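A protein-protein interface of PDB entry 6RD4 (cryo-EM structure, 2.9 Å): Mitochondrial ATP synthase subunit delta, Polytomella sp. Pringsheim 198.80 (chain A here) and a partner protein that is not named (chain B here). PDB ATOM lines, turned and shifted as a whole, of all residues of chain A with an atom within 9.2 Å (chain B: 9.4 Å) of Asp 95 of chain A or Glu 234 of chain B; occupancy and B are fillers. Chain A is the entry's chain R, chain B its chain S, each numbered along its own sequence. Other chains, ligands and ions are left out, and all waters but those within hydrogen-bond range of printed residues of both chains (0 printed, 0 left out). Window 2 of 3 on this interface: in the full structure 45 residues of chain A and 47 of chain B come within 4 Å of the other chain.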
ATOM      1  N   LEU A  91      13.335 -36.499  -9.783  1.00  0.00           N
ATOM      2  CA  LEU A  91      13.497 -36.207 -11.188  1.00  0.00           C
ATOM      3  C   LEU A  91      14.968 -36.151 -11.534  1.00  0.00           C
ATOM      4  O   LEU A  91      15.745 -35.573 -10.771  1.00  0.00           O
ATOM      5  CB  LEU A  91      12.839 -34.880 -11.514  1.00  0.00           C
ATOM      6  CG  LEU A  91      11.330 -34.968 -11.536  1.00  0.00           C
ATOM      7  CD1 LEU A  91      10.732 -33.605 -11.625  1.00  0.00           C
ATOM      8  CD2 LEU A  91      10.941 -35.786 -12.724  1.00  0.00           C
ATOM      9  N   PRO A  92      15.391 -36.724 -12.635  1.00  0.00           N
ATOM     10  CA  PRO A  92      16.826 -36.727 -12.980  1.00  0.00           C
ATOM     11  C   PRO A  92      17.270 -35.519 -13.799  1.00  0.00           C
ATOM     12  O   PRO A  92      17.564 -35.625 -14.989  1.00  0.00           O
ATOM     13  CB  PRO A  92      16.955 -38.028 -13.768  1.00  0.00           C
ATOM     14  CG  PRO A  92      15.634 -38.180 -14.434  1.00  0.00           C
ATOM     15  CD  PRO A  92      14.598 -37.524 -13.576  1.00  0.00           C
ATOM     16  N   GLY A  93      17.360 -34.353 -13.153  1.00  0.00           N
ATOM     17  CA  GLY A  93      17.716 -33.134 -13.858  1.00  0.00           C
ATOM     18  C   GLY A  93      19.146 -33.142 -14.358  1.00  0.00           C
ATOM     19  O   GLY A  93      19.950 -33.994 -13.999  1.00  0.00           O
ATOM     20  N   VAL A  94      19.469 -32.184 -15.229  1.00  0.00           N
ATOM     21  CA  VAL A  94      20.806 -32.178 -15.810  1.00  0.00           C
ATOM     22  C   VAL A  94      21.853 -31.683 -14.830  1.00  0.00           C
ATOM     23  O   VAL A  94      23.037 -31.996 -14.989  1.00  0.00           O
ATOM     24  CB  VAL A  94      20.877 -31.347 -17.101  1.00  0.00           C
ATOM     25  CG1 VAL A  94      20.120 -32.019 -18.201  1.00  0.00           C
ATOM     26  CG2 VAL A  94      20.343 -29.982 -16.869  1.00  0.00           C
ATOM     27  N   ASP A  95      21.461 -30.913 -13.818  1.00  0.00           N
ATOM     28  CA  ASP A  95      22.395 -30.585 -12.753  1.00  0.00           C
ATOM     29  C   ASP A  95      22.576 -31.785 -11.842  1.00  0.00           C
ATOM     30  O   ASP A  95      23.701 -32.171 -11.508  1.00  0.00           O
ATOM     31  CB  ASP A  95      21.893 -29.375 -11.974  1.00  0.00           C
ATOM     32  CG  ASP A  95      21.750 -28.146 -12.844  1.00  0.00           C
ATOM     33  OD1 ASP A  95      21.089 -27.187 -12.406  1.00  0.00           O
ATOM     34  OD2 ASP A  95      22.297 -28.133 -13.965  1.00  0.00           O
ATOM     35  N   GLY A  96      21.470 -32.388 -11.438  1.00  0.00           N
ATOM     36  CA  GLY A  96      21.497 -33.638 -10.709  1.00  0.00           C
ATOM     37  C   GLY A  96      20.089 -34.026 -10.341  1.00  0.00           C
ATOM     38  O   GLY A  96      19.130 -33.322 -10.656  1.00  0.00           O
ATOM     39  N   TYR A  97      19.980 -35.161  -9.658  1.00  0.00           N
ATOM     40  CA  TYR A  97      18.688 -35.664  -9.220  1.00  0.00           C
ATOM     41  C   TYR A  97      18.103 -34.729  -8.181  1.00  0.00           C
ATOM     42  O   TYR A  97      18.699 -34.525  -7.126  1.00  0.00           O
ATOM     43  CB  TYR A  97      18.829 -37.060  -8.628  1.00  0.00           C
ATOM     44  CG  TYR A  97      18.953 -38.174  -9.623  1.00  0.00           C
ATOM     45  CD1 TYR A  97      20.148 -38.411 -10.277  1.00  0.00           C
ATOM     46  CD2 TYR A  97      17.883 -39.001  -9.900  1.00  0.00           C
ATOM     47  CE1 TYR A  97      20.276 -39.427 -11.180  1.00  0.00           C
ATOM     48  CE2 TYR A  97      18.000 -40.023 -10.805  1.00  0.00           C
ATOM     49  CZ  TYR A  97      19.201 -40.230 -11.441  1.00  0.00           C
ATOM     50  OH  TYR A  97      19.334 -41.249 -12.349  1.00  0.00           O
ATOM     51  N   PHE A  98      16.958 -34.147  -8.475  1.00  0.00           N
ATOM     52  CA  PHE A  98      16.257 -33.361  -7.478  1.00  0.00           C
ATOM     53  C   PHE A  98      14.917 -34.002  -7.167  1.00  0.00           C
ATOM     54  O   PHE A  98      14.455 -34.901  -7.862  1.00  0.00           O
ATOM     55  CB  PHE A  98      16.096 -31.906  -7.923  1.00  0.00           C
ATOM     56  CG  PHE A  98      15.233 -31.708  -9.128  1.00  0.00           C
ATOM     57  CD1 PHE A  98      15.738 -31.890 -10.400  1.00  0.00           C
ATOM     58  CD2 PHE A  98      13.938 -31.255  -8.991  1.00  0.00           C
ATOM     59  CE1 PHE A  98      14.960 -31.686 -11.490  1.00  0.00           C
ATOM     60  CE2 PHE A  98      13.157 -31.040 -10.089  1.00  0.00           C
ATOM     61  CZ  PHE A  98      13.670 -31.262 -11.333  1.00  0.00           C
ATOM     62  N   GLY A  99      14.323 -33.562  -6.080  1.00  0.00           N
ATOM     63  CA  GLY A  99      13.043 -34.092  -5.644  1.00  0.00           C
ATOM     64  C   GLY A  99      12.035 -32.976  -5.520  1.00  0.00           C
ATOM     65  O   GLY A  99      12.380 -31.849  -5.182  1.00  0.00           O
ATOM     66  N   HIS A 104       6.337 -26.932  -4.420  1.00  0.00           N
ATOM     67  CA  HIS A 104       7.658 -26.683  -4.983  1.00  0.00           C
ATOM     68  C   HIS A 104       7.672 -25.367  -5.755  1.00  0.00           C
ATOM     69  O   HIS A 104       6.633 -24.832  -6.145  1.00  0.00           O
ATOM     70  CB  HIS A 104       8.039 -27.830  -5.913  1.00  0.00           C
ATOM     71  CG  HIS A 104       9.506 -27.970  -6.183  1.00  0.00           C
ATOM     72  ND1 HIS A 104      10.313 -28.838  -5.481  1.00  0.00           N
ATOM     73  CD2 HIS A 104      10.297 -27.410  -7.128  1.00  0.00           C
ATOM     74  CE1 HIS A 104      11.543 -28.782  -5.960  1.00  0.00           C
ATOM     75  NE2 HIS A 104      11.560 -27.922  -6.960  1.00  0.00           N
ATOM     76  N   VAL A 105       8.867 -24.833  -5.947  1.00  0.00           N
ATOM     77  CA  VAL A 105       9.036 -23.611  -6.738  1.00  0.00           C
ATOM     78  C   VAL A 105       8.726 -23.930  -8.197  1.00  0.00           C
ATOM     79  O   VAL A 105       8.906 -25.085  -8.615  1.00  0.00           O
ATOM     80  CB  VAL A 105      10.461 -23.063  -6.554  1.00  0.00           C
ATOM     81  CG1 VAL A 105      11.498 -24.097  -6.908  1.00  0.00           C
ATOM     82  CG2 VAL A 105      10.715 -21.771  -7.310  1.00  0.00           C
ATOM     83  N   PRO A 106       8.135 -23.008  -8.959  1.00  0.00           N
ATOM     84  CA  PRO A 106       7.971 -23.235 -10.398  1.00  0.00           C
ATOM     85  C   PRO A 106       9.297 -23.487 -11.100  1.00  0.00           C
ATOM     86  O   PRO A 106      10.288 -22.793 -10.870  1.00  0.00           O
ATOM     87  CB  PRO A 106       7.317 -21.943 -10.879  1.00  0.00           C
ATOM     88  CG  PRO A 106       6.525 -21.502  -9.722  1.00  0.00           C
ATOM     89  CD  PRO A 106       7.268 -21.918  -8.485  1.00  0.00           C
ATOM     90  N   THR A 107       9.296 -24.493 -11.971  1.00  0.00           N
ATOM     91  CA  THR A 107      10.513 -25.115 -12.469  1.00  0.00           C
ATOM     92  C   THR A 107      10.283 -25.549 -13.905  1.00  0.00           C
ATOM     93  O   THR A 107       9.230 -26.100 -14.210  1.00  0.00           O
ATOM     94  CB  THR A 107      10.869 -26.317 -11.585  1.00  0.00           C
ATOM     95  OG1 THR A 107      11.229 -25.858 -10.278  1.00  0.00           O
ATOM     96  CG2 THR A 107      12.009 -27.119 -12.146  1.00  0.00           C
ATOM     97  N   ILE A 108      11.233 -25.258 -14.791  1.00  0.00           N
ATOM     98  CA  ILE A 108      11.325 -25.895 -16.099  1.00  0.00           C
ATOM     99  C   ILE A 108      12.647 -26.636 -16.115  1.00  0.00           C
ATOM    100  O   ILE A 108      13.707 -26.017 -16.228  1.00  0.00           O
ATOM    101  CB  ILE A 108      11.250 -24.893 -17.249  1.00  0.00           C
ATOM    102  CG1 ILE A 108       9.890 -24.230 -17.277  1.00  0.00           C
ATOM    103  CG2 ILE A 108      11.483 -25.582 -18.559  1.00  0.00           C
ATOM    104  CD1 ILE A 108       9.817 -23.111 -18.255  1.00  0.00           C
ATOM    105  N   ALA A 109      12.601 -27.950 -15.982  1.00  0.00           N
ATOM    106  CA  ALA A 109      13.802 -28.730 -15.750  1.00  0.00           C
ATOM    107  C   ALA A 109      14.033 -29.664 -16.915  1.00  0.00           C
ATOM    108  O   ALA A 109      13.215 -30.544 -17.171  1.00  0.00           O
ATOM    109  CB  ALA A 109      13.692 -29.523 -14.458  1.00  0.00           C
ATOM    110  N   GLN A 110      15.133 -29.475 -17.619  1.00  0.00           N
ATOM    111  CA  GLN A 110      15.541 -30.440 -18.619  1.00  0.00           C
ATOM    112  C   GLN A 110      16.170 -31.627 -17.923  1.00  0.00           C
ATOM    113  O   GLN A 110      17.058 -31.459 -17.090  1.00  0.00           O
ATOM    114  CB  GLN A 110      16.523 -29.822 -19.602  1.00  0.00           C
ATOM    115  CG  GLN A 110      17.096 -30.820 -20.572  1.00  0.00           C
ATOM    116  CD  GLN A 110      17.979 -30.183 -21.610  1.00  0.00           C
ATOM    117  OE1 GLN A 110      17.898 -28.981 -21.858  1.00  0.00           O
ATOM    118  NE2 GLN A 110      18.834 -30.983 -22.227  1.00  0.00           N
ATOM    119  N   LEU A 111      15.706 -32.825 -18.244  1.00  0.00           N
ATOM    120  CA  LEU A 111      16.153 -34.019 -17.551  1.00  0.00           C
ATOM    121  C   LEU A 111      17.172 -34.791 -18.375  1.00  0.00           C
ATOM    122  O   LEU A 111      17.075 -34.866 -19.600  1.00  0.00           O
ATOM    123  CB  LEU A 111      14.972 -34.917 -17.210  1.00  0.00           C
ATOM    124  CG  LEU A 111      13.819 -34.252 -16.472  1.00  0.00           C
ATOM    125  CD1 LEU A 111      12.737 -35.259 -16.235  1.00  0.00           C
ATOM    126  CD2 LEU A 111      14.268 -33.662 -15.183  1.00  0.00           C
ATOM    127  N   LYS A 112      18.158 -35.346 -17.687  1.00  0.00           N
ATOM    128  CA  LYS A 112      19.099 -36.293 -18.257  1.00  0.00           C
ATOM    129  C   LYS A 112      18.430 -37.643 -18.423  1.00  0.00           C
ATOM    130  O   LYS A 112      17.340 -37.872 -17.904  1.00  0.00           O
ATOM    131  CB  LYS A 112      20.314 -36.425 -17.343  1.00  0.00           C
ATOM    132  CG  LYS A 112      21.428 -35.462 -17.614  1.00  0.00           C
ATOM    133  CD  LYS A 112      22.389 -35.438 -16.446  1.00  0.00           C
ATOM    134  CE  LYS A 112      23.134 -36.732 -16.272  1.00  0.00           C
ATOM    135  NZ  LYS A 112      24.116 -36.595 -15.165  1.00  0.00           N
ATOM    136  N   GLY A 132      14.183 -35.533 -21.401  1.00  0.00           N
ATOM    137  CA  GLY A 132      12.985 -34.821 -21.780  1.00  0.00           C
ATOM    138  C   GLY A 132      12.480 -34.130 -20.546  1.00  0.00           C
ATOM    139  O   GLY A 132      12.583 -34.633 -19.451  1.00  0.00           O
ATOM    140  N   PHE A 133      11.854 -32.988 -20.755  1.00  0.00           N
ATOM    141  CA  PHE A 133      11.705 -31.967 -19.741  1.00  0.00           C
ATOM    142  C   PHE A 133      10.698 -32.375 -18.679  1.00  0.00           C
ATOM    143  O   PHE A 133       9.981 -33.362 -18.804  1.00  0.00           O
ATOM    144  CB  PHE A 133      11.275 -30.662 -20.384  1.00  0.00           C
ATOM    145  CG  PHE A 133      12.166 -30.229 -21.491  1.00  0.00           C
ATOM    146  CD1 PHE A 133      13.288 -29.486 -21.226  1.00  0.00           C
ATOM    147  CD2 PHE A 133      11.886 -30.566 -22.797  1.00  0.00           C
ATOM    148  CE1 PHE A 133      14.121 -29.100 -22.237  1.00  0.00           C
ATOM    149  CE2 PHE A 133      12.701 -30.166 -23.804  1.00  0.00           C
ATOM    150  CZ  PHE A 133      13.825 -29.437 -23.526  1.00  0.00           C
ATOM    151  N   ALA A 134      10.670 -31.592 -17.607  1.00  0.00           N
ATOM    152  CA  ALA A 134       9.707 -31.761 -16.530  1.00  0.00           C
ATOM    153  C   ALA A 134       9.389 -30.383 -15.992  1.00  0.00           C
ATOM    154  O   ALA A 134      10.291 -29.684 -15.536  1.00  0.00           O
ATOM    155  CB  ALA A 134      10.260 -32.640 -15.420  1.00  0.00           C
ATOM    156  N   PHE A 135       8.129 -29.986 -16.033  1.00  0.00           N
ATOM    157  CA  PHE A 135       7.739 -28.667 -15.575  1.00  0.00           C
ATOM    158  C   PHE A 135       6.981 -28.808 -14.271  1.00  0.00           C
ATOM    159  O   PHE A 135       6.115 -29.675 -14.146  1.00  0.00           O
ATOM    160  CB  PHE A 135       6.867 -27.919 -16.582  1.00  0.00           C
ATOM    161  CG  PHE A 135       7.172 -28.226 -18.002  1.00  0.00           C
ATOM    162  CD1 PHE A 135       8.422 -27.990 -18.525  1.00  0.00           C
ATOM    163  CD2 PHE A 135       6.192 -28.723 -18.829  1.00  0.00           C
ATOM    164  CE1 PHE A 135       8.697 -28.277 -19.832  1.00  0.00           C
ATOM    165  CE2 PHE A 135       6.462 -29.008 -20.141  1.00  0.00           C
ATOM    166  CZ  PHE A 135       7.715 -28.782 -20.642  1.00  0.00           C
ATOM    167  N   TYR B 231       9.158 -19.456 -13.567  1.00  0.00           N
ATOM    168  CA  TYR B 231       9.772 -20.771 -13.533  1.00  0.00           C
ATOM    169  C   TYR B 231      11.275 -20.665 -13.391  1.00  0.00           C
ATOM    170  O   TYR B 231      11.921 -19.859 -14.061  1.00  0.00           O
ATOM    171  CB  TYR B 231       9.453 -21.551 -14.805  1.00  0.00           C
ATOM    172  CG  TYR B 231       7.989 -21.758 -15.059  1.00  0.00           C
ATOM    173  CD1 TYR B 231       7.331 -22.857 -14.541  1.00  0.00           C
ATOM    174  CD2 TYR B 231       7.270 -20.860 -15.817  1.00  0.00           C
ATOM    175  CE1 TYR B 231       6.006 -23.048 -14.770  1.00  0.00           C
ATOM    176  CE2 TYR B 231       5.947 -21.042 -16.043  1.00  0.00           C
ATOM    177  CZ  TYR B 231       5.321 -22.135 -15.520  1.00  0.00           C
ATOM    178  OH  TYR B 231       3.985 -22.311 -15.761  1.00  0.00           O
ATOM    179  N   ASP B 232      11.831 -21.523 -12.554  1.00  0.00           N
ATOM    180  CA  ASP B 232      13.265 -21.572 -12.352  1.00  0.00           C
ATOM    181  C   ASP B 232      13.842 -22.552 -13.362  1.00  0.00           C
ATOM    182  O   ASP B 232      13.559 -23.750 -13.297  1.00  0.00           O
ATOM    183  CB  ASP B 232      13.570 -21.993 -10.915  1.00  0.00           C
ATOM    184  CG  ASP B 232      14.985 -21.671 -10.492  1.00  0.00           C
ATOM    185  OD1 ASP B 232      15.749 -21.110 -11.303  1.00  0.00           O
ATOM    186  OD2 ASP B 232      15.333 -21.982  -9.337  1.00  0.00           O
ATOM    187  N   ILE B 233      14.646 -22.047 -14.292  1.00  0.00           N
ATOM    188  CA  ILE B 233      15.145 -22.875 -15.384  1.00  0.00           C
ATOM    189  C   ILE B 233      16.267 -23.760 -14.871  1.00  0.00           C
ATOM    190  O   ILE B 233      17.247 -23.276 -14.298  1.00  0.00           O
ATOM    191  CB  ILE B 233      15.627 -22.014 -16.554  1.00  0.00           C
ATOM    192  CG1 ILE B 233      14.574 -20.985 -16.929  1.00  0.00           C
ATOM    193  CG2 ILE B 233      15.943 -22.881 -17.741  1.00  0.00           C
ATOM    194  CD1 ILE B 233      13.278 -21.579 -17.370  1.00  0.00           C
ATOM    195  N   GLU B 234      16.135 -25.063 -15.082  1.00  0.00           N
ATOM    196  CA  GLU B 234      17.152 -26.023 -14.687  1.00  0.00           C
ATOM    197  C   GLU B 234      17.854 -26.609 -15.905  1.00  0.00           C
ATOM    198  O   GLU B 234      18.108 -27.806 -15.963  1.00  0.00           O
ATOM    199  CB  GLU B 234      16.503 -27.104 -13.819  1.00  0.00           C
ATOM    200  CG  GLU B 234      17.397 -27.872 -12.846  1.00  0.00           C
ATOM    201  CD  GLU B 234      17.781 -29.245 -13.349  1.00  0.00           C
ATOM    202  OE1 GLU B 234      17.004 -29.840 -14.112  1.00  0.00           O
ATOM    203  OE2 GLU B 234      18.861 -29.734 -12.991  1.00  0.00           O
ATOM    204  N   ALA B 235      18.142 -25.796 -16.905  1.00  0.00           N
ATOM    205  CA  ALA B 235      18.755 -26.355 -18.094  1.00  0.00           C
ATOM    206  C   ALA B 235      20.267 -26.289 -18.011  1.00  0.00           C
ATOM    207  O   ALA B 235      20.846 -25.758 -17.065  1.00  0.00           O
ATOM    208  CB  ALA B 235      18.279 -25.625 -19.341  1.00  0.00           C
ATOM    209  N   SER B 236      20.912 -26.842 -19.032  1.00  0.00           N
ATOM    210  CA  SER B 236      22.354 -26.694 -19.158  1.00  0.00           C
ATOM    211  C   SER B 236      22.724 -25.268 -19.541  1.00  0.00           C
ATOM    212  O   SER B 236      23.549 -24.630 -18.883  1.00  0.00           O
ATOM    213  CB  SER B 236      22.888 -27.679 -20.191  1.00  0.00           C
ATOM    214  OG  SER B 236      24.268 -27.474 -20.409  1.00  0.00           O
ATOM    215  N   HIS B 237      22.135 -24.761 -20.608  1.00  0.00           N
ATOM    216  CA  HIS B 237      22.386 -23.446 -21.142  1.00  0.00           C
ATOM    217  C   HIS B 237      21.215 -22.513 -20.840  1.00  0.00           C
ATOM    218  O   HIS B 237      20.456 -22.745 -19.896  1.00  0.00           O
ATOM    219  CB  HIS B 237      22.713 -23.589 -22.613  1.00  0.00           C
ATOM    220  CG  HIS B 237      24.017 -24.270 -22.851  1.00  0.00           C
ATOM    221  ND1 HIS B 237      24.193 -25.622 -22.662  1.00  0.00           N
ATOM    222  CD2 HIS B 237      25.220 -23.783 -23.229  1.00  0.00           C
ATOM    223  CE1 HIS B 237      25.445 -25.942 -22.930  1.00  0.00           C
ATOM    224  NE2 HIS B 237      26.088 -24.846 -23.280  1.00  0.00           N
ATOM    225  N   GLU B 238      21.121 -21.422 -21.592  1.00  0.00           N
ATOM    226  CA  GLU B 238      20.250 -20.307 -21.256  1.00  0.00           C
ATOM    227  C   GLU B 238      18.777 -20.669 -21.403  1.00  0.00           C
ATOM    228  O   GLU B 238      18.407 -21.695 -21.974  1.00  0.00           O
ATOM    229  CB  GLU B 238      20.549 -19.107 -22.145  1.00  0.00           C
ATOM    230  CG  GLU B 238      22.017 -18.789 -22.318  1.00  0.00           C
ATOM    231  CD  GLU B 238      22.774 -18.813 -21.014  1.00  0.00           C
ATOM    232  OE1 GLU B 238      23.739 -19.597 -20.912  1.00  0.00           O
ATOM    233  OE2 GLU B 238      22.385 -18.070 -20.090  1.00  0.00           O
ATOM    234  N   ARG B 239      17.932 -19.783 -20.873  1.00  0.00           N
ATOM    235  CA  ARG B 239      16.492 -19.930 -21.030  1.00  0.00           C
ATOM    236  C   ARG B 239      16.080 -19.767 -22.482  1.00  0.00           C
ATOM    237  O   ARG B 239      15.193 -20.477 -22.968  1.00  0.00           O
ATOM    238  CB  ARG B 239      15.764 -18.906 -20.170  1.00  0.00           C
ATOM    239  CG  ARG B 239      14.276 -19.076 -20.180  1.00  0.00           C
ATOM    240  CD  ARG B 239      13.612 -18.064 -19.318  1.00  0.00           C
ATOM    241  NE  ARG B 239      13.674 -16.748 -19.928  1.00  0.00           N
ATOM    242  CZ  ARG B 239      12.925 -15.727 -19.544  1.00  0.00           C
ATOM    243  NH1 ARG B 239      12.064 -15.883 -18.550  1.00  0.00           N
ATOM    244  NH2 ARG B 239      13.038 -14.557 -20.149  1.00  0.00           N
ATOM    245  N   VAL B 242      16.928 -23.229 -23.902  1.00  0.00           N
ATOM    246  CA  VAL B 242      16.062 -24.345 -23.562  1.00  0.00           C
ATOM    247  C   VAL B 242      14.721 -24.183 -24.257  1.00  0.00           C
ATOM    248  O   VAL B 242      14.113 -25.175 -24.655  1.00  0.00           O
ATOM    249  CB  VAL B 242      15.928 -24.509 -22.029  1.00  0.00           C
ATOM    250  CG1 VAL B 242      15.117 -23.422 -21.387  1.00  0.00           C
ATOM    251  CG2 VAL B 242      15.323 -25.811 -21.683  1.00  0.00           C
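N of Asp 95 of chain A sits at hydrogen-bond distance from OE2 of Glu 234 of chain B (3.0 Å). The backbone NH (N) of Ile 108 of chain A lies within hydrogen-bond range of the backbone carbonyl oxygen (O) of Asp 232 of chain B (3.1 Å). The backbone NH (N) of Glu 234 of chain B is in hydrogen-bond range of the backbone carbonyl oxygen (O) of Ile 108 of chain A, 2.8 Å away. The side-chain carboxylate of Glu 234 of chain B sits at hydrogen-bond distance from the backbone NH of Val 94 of chain A (3.4 Å). OE1 of Glu 234 of chain B lies close to O of Gln 110 of chain A (3.4 Å). N of Asp 232 of chain B is in hydrogen-bond range of O of Pro 106 of chain A (2.6 Å).
The backbone NH (N) of Leu 91 of chain A is in hydrogen-bond range of the backbone carbonyl oxygen (O) of Phe 98 of chain A, 2.7 Å away. N of Val 94 of chain A sits at hydrogen-bond distance from O of Gln 110 of chain A (3.1 Å). A ring nitrogen (ND1) of His 237 of chain B is in hydrogen-bond range of the side-chain hydroxyl of Ser 236 of chain B (2.9 Å). O of Val 105 of chain A sits at hydrogen-bond distance from OG1 of Thr 107 of chain A (3.0 Å). The backbone NH (N) of Ala 134 of chain A lies within hydrogen-bond range of the backbone carbonyl oxygen (O) of Ala 109 of chain A.
Glu 234 of chain B touches Gly 93 of chain A (OE1 to CA, 3.4 Å). Val 94 of chain A touches Ala 235 of chain B. Ser 236 of chain B touches Val 94 of chain A. OE1 of Glu 234 of chain B touches CE1 of Phe 98 of chain A, 3.8 Å away. Tyr 231 of chain B touches Pro 106 of chain A. Thr 107 of chain A touches Tyr 231 of chain B. Tyr 231 of chain B touches Ile 108 of chain A. Ile 108 of chain A touches Ile 233 of chain B (O to CA, 3.6 Å). Glu 234 of chain B touches Ala 109 of chain A. Val 242 of chain B touches Phe 133 of chain A.
Gly 93 of chain A touches just one residue of chain B: Glu 234. Val 94 of chain A touches just these residues of chain B: Glu 234, Ala 235 and Ser 236. Asp 95 of chain A touches just one residue of chain B: Glu 234 (3.0 Å). No residue of chain B comes within 4 Å of Gly 96 of chain A. Printed residues of chain B within 4 Å of Thr 107 of chain A: Tyr 231 and Asp 232. Printed residues of chain B within 4 Å of Ile 108 of chain A: Tyr 231, Asp 232, Ile 233 and Glu 234. Glu 234 of chain B touches just these residues of chain A: Gly 93 (3.4 Å), Val 94 (3.2 Å), Asp 95 (3.0 Å), Phe 98 (3.8 Å), Ile 108 (2.8 Å), Ala 109 (3.3 Å) and Gln 110 (3.4 Å). The nearest residue of chain B that does not touch Asp 95 of chain A is Ala 235 of chain B (4.2 Å).
Of the 22 printed residues of chain A, 10 touch a printed residue of chain B. Hydrophobic or aromatic side chains of chain A that line the printed part of chain B: Val 94, Phe 98, Pro 106, Ile 108, Ala 109 and Phe 133. Among the printed residues, 17 pairs touch across the chains. Among the printed residues, no Asp or Glu carboxylate lies within 4 Å of a Lys or Arg side-chain nitrogen of the other chain.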
